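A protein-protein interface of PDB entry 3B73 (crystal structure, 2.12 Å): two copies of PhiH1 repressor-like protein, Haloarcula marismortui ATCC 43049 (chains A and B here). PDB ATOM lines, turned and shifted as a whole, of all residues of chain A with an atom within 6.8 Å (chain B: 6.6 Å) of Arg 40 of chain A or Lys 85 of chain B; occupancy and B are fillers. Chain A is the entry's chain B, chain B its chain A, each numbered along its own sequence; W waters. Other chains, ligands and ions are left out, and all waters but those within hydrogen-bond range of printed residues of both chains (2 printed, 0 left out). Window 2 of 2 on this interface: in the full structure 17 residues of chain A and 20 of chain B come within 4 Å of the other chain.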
ATOM      1  N   TRP A  14     -16.240 -32.289  22.591  1.00  0.00           N
ATOM      2  CA  TRP A  14     -14.977 -31.916  21.972  1.00  0.00           C
ATOM      3  C   TRP A  14     -14.256 -33.139  21.459  1.00  0.00           C
ATOM      4  O   TRP A  14     -13.461 -33.058  20.527  1.00  0.00           O
ATOM      5  CB  TRP A  14     -14.115 -31.076  22.937  1.00  0.00           C
ATOM      6  CG  TRP A  14     -14.932 -29.908  23.429  1.00  0.00           C
ATOM      7  CD1 TRP A  14     -15.435 -29.729  24.690  1.00  0.00           C
ATOM      8  CD2 TRP A  14     -15.442 -28.817  22.633  1.00  0.00           C
ATOM      9  NE1 TRP A  14     -16.202 -28.575  24.727  1.00  0.00           N
ATOM     10  CE2 TRP A  14     -16.212 -27.999  23.483  1.00  0.00           C
ATOM     11  CE3 TRP A  14     -15.289 -28.440  21.297  1.00  0.00           C
ATOM     12  CZ2 TRP A  14     -16.837 -26.826  23.035  1.00  0.00           C
ATOM     13  CZ3 TRP A  14     -15.921 -27.285  20.856  1.00  0.00           C
ATOM     14  CH2 TRP A  14     -16.681 -26.493  21.725  1.00  0.00           C
ATOM     15  N   LEU A  33      -4.549 -28.307  17.315  1.00  0.00           N
ATOM     16  CA  LEU A  33      -5.984 -28.522  17.517  1.00  0.00           C
ATOM     17  C   LEU A  33      -6.597 -27.323  18.222  1.00  0.00           C
ATOM     18  O   LEU A  33      -7.693 -26.865  17.862  1.00  0.00           O
ATOM     19  CB  LEU A  33      -6.235 -29.795  18.319  1.00  0.00           C
ATOM     20  CG  LEU A  33      -6.172 -31.075  17.485  1.00  0.00           C
ATOM     21  CD1 LEU A  33      -6.062 -32.278  18.405  1.00  0.00           C
ATOM     22  CD2 LEU A  33      -7.400 -31.179  16.563  1.00  0.00           C
ATOM     23  N   GLU A  34      -5.875 -26.840  19.234  1.00  0.00           N
ATOM     24  CA  GLU A  34      -6.209 -25.624  19.982  1.00  0.00           C
ATOM     25  C   GLU A  34      -6.525 -24.440  19.054  1.00  0.00           C
ATOM     26  O   GLU A  34      -7.460 -23.661  19.283  1.00  0.00           O
ATOM     27  CB  GLU A  34      -5.032 -25.278  20.912  1.00  0.00           C
ATOM     28  CG  GLU A  34      -5.111 -23.919  21.547  1.00  0.00           C
ATOM     29  CD  GLU A  34      -6.392 -23.750  22.310  1.00  0.00           C
ATOM     30  OE1 GLU A  34      -6.849 -24.753  22.896  1.00  0.00           O
ATOM     31  OE2 GLU A  34      -6.947 -22.630  22.313  1.00  0.00           O
ATOM     32  N   ARG A  36      -7.751 -24.355  16.092  1.00  0.00           N
ATOM     33  CA  ARG A  36      -8.951 -24.476  15.266  1.00  0.00           C
ATOM     34  C   ARG A  36     -10.118 -23.652  15.834  1.00  0.00           C
ATOM     35  O   ARG A  36     -10.261 -23.523  17.055  1.00  0.00           O
ATOM     36  CB  ARG A  36      -9.349 -25.941  15.170  1.00  0.00           C
ATOM     37  CG  ARG A  36      -8.439 -26.753  14.297  1.00  0.00           C
ATOM     38  CD  ARG A  36      -8.706 -26.383  12.862  1.00  0.00           C
ATOM     39  NE  ARG A  36      -8.767 -27.575  12.024  1.00  0.00           N
ATOM     40  CZ  ARG A  36      -9.783 -27.868  11.216  1.00  0.00           C
ATOM     41  NH1 ARG A  36      -9.764 -28.979  10.486  1.00  0.00           N
ATOM     42  NH2 ARG A  36     -10.810 -27.040  11.121  1.00  0.00           N
ATOM     43  N   ASP A  37     -10.957 -23.092  14.963  1.00  0.00           N
ATOM     44  CA  ASP A  37     -12.099 -22.300  15.437  1.00  0.00           C
ATOM     45  C   ASP A  37     -13.070 -23.195  16.185  1.00  0.00           C
ATOM     46  O   ASP A  37     -13.743 -22.769  17.131  1.00  0.00           O
ATOM     47  CB  ASP A  37     -12.836 -21.634  14.272  1.00  0.00           C
ATOM     48  CG  ASP A  37     -12.158 -20.359  13.799  1.00  0.00           C
ATOM     49  OD1 ASP A  37     -10.933 -20.217  14.007  1.00  0.00           O
ATOM     50  OD2 ASP A  37     -12.852 -19.499  13.213  1.00  0.00           O
ATOM     51  N   GLU A  38     -13.113 -24.444  15.739  1.00  0.00           N
ATOM     52  CA  GLU A  38     -14.090 -25.419  16.183  1.00  0.00           C
ATOM     53  C   GLU A  38     -13.757 -25.992  17.544  1.00  0.00           C
ATOM     54  O   GLU A  38     -14.573 -26.704  18.136  1.00  0.00           O
ATOM     55  CB  GLU A  38     -14.178 -26.564  15.168  1.00  0.00           C
ATOM     56  CG  GLU A  38     -14.611 -26.112  13.795  1.00  0.00           C
ATOM     57  CD  GLU A  38     -13.435 -25.855  12.880  1.00  0.00           C
ATOM     58  OE1 GLU A  38     -12.309 -25.668  13.389  1.00  0.00           O
ATOM     59  OE2 GLU A  38     -13.639 -25.859  11.649  1.00  0.00           O
ATOM     60  N   ILE A  39     -12.544 -25.724  18.019  1.00  0.00           N
ATOM     61  CA  ILE A  39     -12.147 -26.198  19.338  1.00  0.00           C
ATOM     62  C   ILE A  39     -12.230 -25.040  20.325  1.00  0.00           C
ATOM     63  O   ILE A  39     -11.517 -24.053  20.179  1.00  0.00           O
ATOM     64  CB  ILE A  39     -10.735 -26.788  19.320  1.00  0.00           C
ATOM     65  CG1 ILE A  39     -10.646 -27.953  18.315  1.00  0.00           C
ATOM     66  CG2 ILE A  39     -10.308 -27.228  20.731  1.00  0.00           C
ATOM     67  CD1 ILE A  39     -11.717 -29.034  18.479  1.00  0.00           C
ATOM     68  N   ARG A  40     -13.121 -25.146  21.307  1.00  0.00           N
ATOM     69  CA  ARG A  40     -13.309 -24.071  22.287  1.00  0.00           C
ATOM     70  C   ARG A  40     -12.859 -24.501  23.688  1.00  0.00           C
ATOM     71  O   ARG A  40     -13.383 -24.026  24.695  1.00  0.00           O
ATOM     72  CB  ARG A  40     -14.780 -23.650  22.320  1.00  0.00           C
ATOM     73  CG  ARG A  40     -15.441 -23.542  20.936  1.00  0.00           C
ATOM     74  CD  ARG A  40     -14.920 -22.340  20.168  1.00  0.00           C
ATOM     75  NE  ARG A  40     -15.100 -21.131  20.958  1.00  0.00           N
ATOM     76  CZ  ARG A  40     -14.428 -19.997  20.778  1.00  0.00           C
ATOM     77  NH1 ARG A  40     -13.510 -19.902  19.824  1.00  0.00           N
ATOM     78  NH2 ARG A  40     -14.672 -18.956  21.561  1.00  0.00           N
ATOM     79  N   ILE A  41     -11.921 -25.437  23.755  1.00  0.00           N
ATOM     80  CA  ILE A  41     -11.304 -25.784  25.027  1.00  0.00           C
ATOM     81  C   ILE A  41      -9.809 -25.498  24.927  1.00  0.00           C
ATOM     82  O   ILE A  41      -9.284 -25.301  23.818  1.00  0.00           O
ATOM     83  CB  ILE A  41     -11.555 -27.254  25.442  1.00  0.00           C
ATOM     84  CG1 ILE A  41     -11.135 -28.215  24.331  1.00  0.00           C
ATOM     85  CG2 ILE A  41     -13.039 -27.469  25.771  1.00  0.00           C
ATOM     86  CD1 ILE A  41     -11.121 -29.683  24.743  1.00  0.00           C
ATOM     87  N   SER A  42      -9.138 -25.464  26.079  1.00  0.00           N
ATOM     88  CA  SER A  42      -7.717 -25.096  26.172  1.00  0.00           C
ATOM     89  C   SER A  42      -6.776 -26.196  25.686  1.00  0.00           C
ATOM     90  O   SER A  42      -7.147 -27.383  25.594  1.00  0.00           O
ATOM     91  CB  SER A  42      -7.350 -24.738  27.619  1.00  0.00           C
ATOM     92  OG  SER A  42      -7.328 -25.905  28.443  1.00  0.00           O
ATOM     93  N   GLN B   6     -19.903 -26.116  14.682  1.00  0.00           N
ATOM     94  CA  GLN B   6     -19.252 -25.119  15.518  1.00  0.00           C
ATOM     95  C   GLN B   6     -19.986 -25.067  16.870  1.00  0.00           C
ATOM     96  O   GLN B   6     -20.940 -24.316  17.041  1.00  0.00           O
ATOM     97  CB  GLN B   6     -19.284 -23.756  14.789  1.00  0.00           C
ATOM     98  CG  GLN B   6     -18.670 -22.618  15.545  1.00  0.00           C
ATOM     99  CD  GLN B   6     -17.181 -22.798  15.753  1.00  0.00           C
ATOM    100  OE1 GLN B   6     -16.470 -23.243  14.848  1.00  0.00           O
ATOM    101  NE2 GLN B   6     -16.698 -22.450  16.951  1.00  0.00           N
ATOM    102  N   SER B   7     -19.551 -25.895  17.820  1.00  0.00           N
ATOM    103  CA  SER B   7     -20.306 -26.090  19.057  1.00  0.00           C
ATOM    104  C   SER B   7     -20.029 -24.999  20.078  1.00  0.00           C
ATOM    105  O   SER B   7     -19.055 -24.276  19.957  1.00  0.00           O
ATOM    106  CB  SER B   7     -19.970 -27.451  19.673  1.00  0.00           C
ATOM    107  OG  SER B   7     -20.186 -28.512  18.753  1.00  0.00           O
ATOM    108  N   GLY B   8     -20.877 -24.898  21.096  1.00  0.00           N
ATOM    109  CA  GLY B   8     -20.675 -23.952  22.187  1.00  0.00           C
ATOM    110  C   GLY B   8     -20.083 -24.629  23.413  1.00  0.00           C
ATOM    111  O   GLY B   8     -20.253 -25.847  23.616  1.00  0.00           O
ATOM    112  N   SER B   9     -19.408 -23.845  24.244  1.00  0.00           N
ATOM    113  CA  SER B   9     -18.771 -24.355  25.466  1.00  0.00           C
ATOM    114  C   SER B   9     -19.770 -25.003  26.426  1.00  0.00           C
ATOM    115  O   SER B   9     -19.389 -25.797  27.279  1.00  0.00           O
ATOM    116  CB  SER B   9     -18.028 -23.237  26.194  1.00  0.00           C
ATOM    117  OG  SER B   9     -17.492 -22.292  25.276  1.00  0.00           O
ATOM    118  N   TYR B  81     -24.154 -22.592  11.724  1.00  0.00           N
ATOM    119  CA  TYR B  81     -24.552 -21.801  12.880  1.00  0.00           C
ATOM    120  C   TYR B  81     -23.570 -21.987  14.050  1.00  0.00           C
ATOM    121  O   TYR B  81     -23.227 -23.106  14.427  1.00  0.00           O
ATOM    122  CB  TYR B  81     -26.003 -22.103  13.280  1.00  0.00           C
ATOM    123  CG  TYR B  81     -26.519 -21.159  14.365  1.00  0.00           C
ATOM    124  CD1 TYR B  81     -27.052 -19.913  14.039  1.00  0.00           C
ATOM    125  CD2 TYR B  81     -26.438 -21.504  15.722  1.00  0.00           C
ATOM    126  CE1 TYR B  81     -27.504 -19.040  15.031  1.00  0.00           C
ATOM    127  CE2 TYR B  81     -26.887 -20.649  16.715  1.00  0.00           C
ATOM    128  CZ  TYR B  81     -27.409 -19.417  16.367  1.00  0.00           C
ATOM    129  OH  TYR B  81     -27.838 -18.583  17.366  1.00  0.00           O
ATOM    130  N   ASP B  82     -23.091 -20.886  14.599  1.00  0.00           N
ATOM    131  CA  ASP B  82     -22.133 -20.943  15.708  1.00  0.00           C
ATOM    132  C   ASP B  82     -22.887 -20.975  17.051  1.00  0.00           C
ATOM    133  O   ASP B  82     -23.388 -19.947  17.519  1.00  0.00           O
ATOM    134  CB  ASP B  82     -21.176 -19.736  15.653  1.00  0.00           C
ATOM    135  CG  ASP B  82     -20.095 -19.794  16.732  1.00  0.00           C
ATOM    136  OD1 ASP B  82     -18.996 -19.262  16.498  1.00  0.00           O
ATOM    137  OD2 ASP B  82     -20.343 -20.377  17.816  1.00  0.00           O
ATOM    138  N   ALA B  83     -22.973 -22.156  17.659  1.00  0.00           N
ATOM    139  CA  ALA B  83     -23.756 -22.349  18.889  1.00  0.00           C
ATOM    140  C   ALA B  83     -23.141 -21.689  20.157  1.00  0.00           C
ATOM    141  O   ALA B  83     -23.795 -21.610  21.210  1.00  0.00           O
ATOM    142  CB  ALA B  83     -23.992 -23.846  19.123  1.00  0.00           C
ATOM    143  N   GLY B  84     -21.888 -21.248  20.046  1.00  0.00           N
ATOM    144  CA  GLY B  84     -21.162 -20.567  21.112  1.00  0.00           C
ATOM    145  C   GLY B  84     -21.342 -19.056  21.080  1.00  0.00           C
ATOM    146  O   GLY B  84     -21.756 -18.461  22.077  1.00  0.00           O
ATOM    147  N   LYS B  85     -21.037 -18.422  19.951  1.00  0.00           N
ATOM    148  CA  LYS B  85     -21.290 -16.966  19.821  1.00  0.00           C
ATOM    149  C   LYS B  85     -22.767 -16.718  19.501  1.00  0.00           C
ATOM    150  O   LYS B  85     -23.268 -15.590  19.600  1.00  0.00           O
ATOM    151  CB  LYS B  85     -20.378 -16.333  18.755  1.00  0.00           C
ATOM    152  CG  LYS B  85     -18.890 -16.592  19.000  1.00  0.00           C
ATOM    153  CD  LYS B  85     -17.989 -15.700  18.156  1.00  0.00           C
ATOM    154  CE  LYS B  85     -16.626 -16.345  17.920  1.00  0.00           C
ATOM    155  NZ  LYS B  85     -16.311 -17.354  18.978  1.00  0.00           N
ATOM    156  N   GLU B  86     -23.473 -17.799  19.161  1.00  0.00           N
ATOM    157  CA  GLU B  86     -24.898 -17.731  18.823  1.00  0.00           C
ATOM    158  C   GLU B  86     -25.131 -16.814  17.606  1.00  0.00           C
ATOM    159  O   GLU B  86     -25.776 -15.783  17.695  1.00  0.00           O
ATOM    160  CB  GLU B  86     -25.747 -17.335  20.059  1.00  0.00           C
ATOM    161  CG  GLU B  86     -25.375 -18.191  21.288  1.00  0.00           C
ATOM    162  CD  GLU B  86     -26.243 -17.959  22.515  1.00  0.00           C
ATOM    163  OE1 GLU B  86     -26.071 -18.720  23.497  1.00  0.00           O
ATOM    164  OE2 GLU B  86     -27.076 -17.026  22.511  1.00  0.00           O
ATOM    165  N   ARG B  87     -24.574 -17.200  16.467  1.00  0.00           N
ATOM    166  CA  ARG B  87     -24.807 -16.462  15.239  1.00  0.00           C
ATOM    167  C   ARG B  87     -24.566 -17.362  14.047  1.00  0.00           C
ATOM    168  O   ARG B  87     -23.764 -18.297  14.127  1.00  0.00           O
ATOM    169  CB  ARG B  87     -23.873 -15.256  15.148  1.00  0.00           C
ATOM    170  CG  ARG B  87     -22.395 -15.568  15.340  1.00  0.00           C
ATOM    171  CD  ARG B  87     -21.525 -14.679  14.442  1.00  0.00           C
ATOM    172  NE  ARG B  87     -20.392 -14.075  15.143  1.00  0.00           N
ATOM    173  CZ  ARG B  87     -19.206 -13.829  14.586  1.00  0.00           C
ATOM    174  NH1 ARG B  87     -18.233 -13.260  15.299  1.00  0.00           N
ATOM    175  NH2 ARG B  87     -18.987 -14.162  13.318  1.00  0.00           N
HETATM  176  O   HOH W   1     -18.112 -21.232  19.551  1.00  0.00           O
HETATM  177  O   HOH W   2     -17.244 -27.212  17.351  1.00  0.00           O
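NZ of Lys 85 of chain B sits close to NH2 of Arg 40 of chain A (3.5 Å).
O of Asp 37 of chain A sits at hydrogen-bond distance from NE2 of Gln 6 of chain B.
Hydrophobic or aromatic side chains of chain A that line the printed part of chain B: Trp 14.
Printed residues of chain B that touch a printed residue of chain A: Gln 6, Ser 7, Gly 8, Ser 9 and Lys 85.
No position is printed for both chains.
Of the printed residues of chain B, Trp 14 of chain A touches Ser 7 (3.7 Å), Gly 8 (3.6 Å) and Ser 9 (3.97 Å).
Of the printed residues of chain B, Glu 38 of chain A touches Gln 6 (3.5 Å).
Arg 40 of chain A touches just these residues of chain B: Gln 6, Ser 7 and Lys 85.
Printed residues of chain A within 4 Å of Gln 6 of chain B: Asp 37, Glu 38 and Arg 40.
Of the printed residues of chain A, Gly 8 of chain B touches Trp 14 (3.6 Å).
Of the printed residues of chain A, Ser 9 of chain B touches Trp 14.
Of the printed residues of chain A, Lys 85 of chain B touches Arg 40 (3.5 Å).
The nearest printed residue of chain A that does not touch Gln 6 of chain B is Ile 39 of chain A (5.4 Å).
Water W2 lies within hydrogen-bond range of N of Ser 7 of chain B (2.7 Å) and O of Glu 38 of chain A (2.8 Å).
Water W1 lies within hydrogen-bond range of OD2 of Asp 82 of chain B (3.0 Å), NE2 of Gln 6 of chain B (3.2 Å), O of Ser 7 of chain B (3.2 Å) and NE of Arg 40 of chain A (3.3 Å).
O of Gln 6 of chain B is in hydrogen-bond range of N of Ala 83 of chain B (3.0 Å).
NH2 of Arg 36 of chain A is in salt-bridge range of OE1 of Glu 38 of chain A, 3.0 Å away.
The backbone NH (N) of Lys 85 of chain B is in hydrogen-bond range of the side-chain carboxylate (OD2) of Asp 82 of chain B, 3.0 Å away.
Among the printed residues, merely in contact across the chains: Trp 14 of chain A with Ser 7 of chain B, Trp 14 of chain A with Gly 8 of chain B, Trp 14 of chain A with Ser 9 of chain B, Glu 38 of chain A with Gln 6 of chain B, Arg 40 of chain A with Gln 6 of chain B and Arg 40 of chain A with Ser 7 of chain B.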
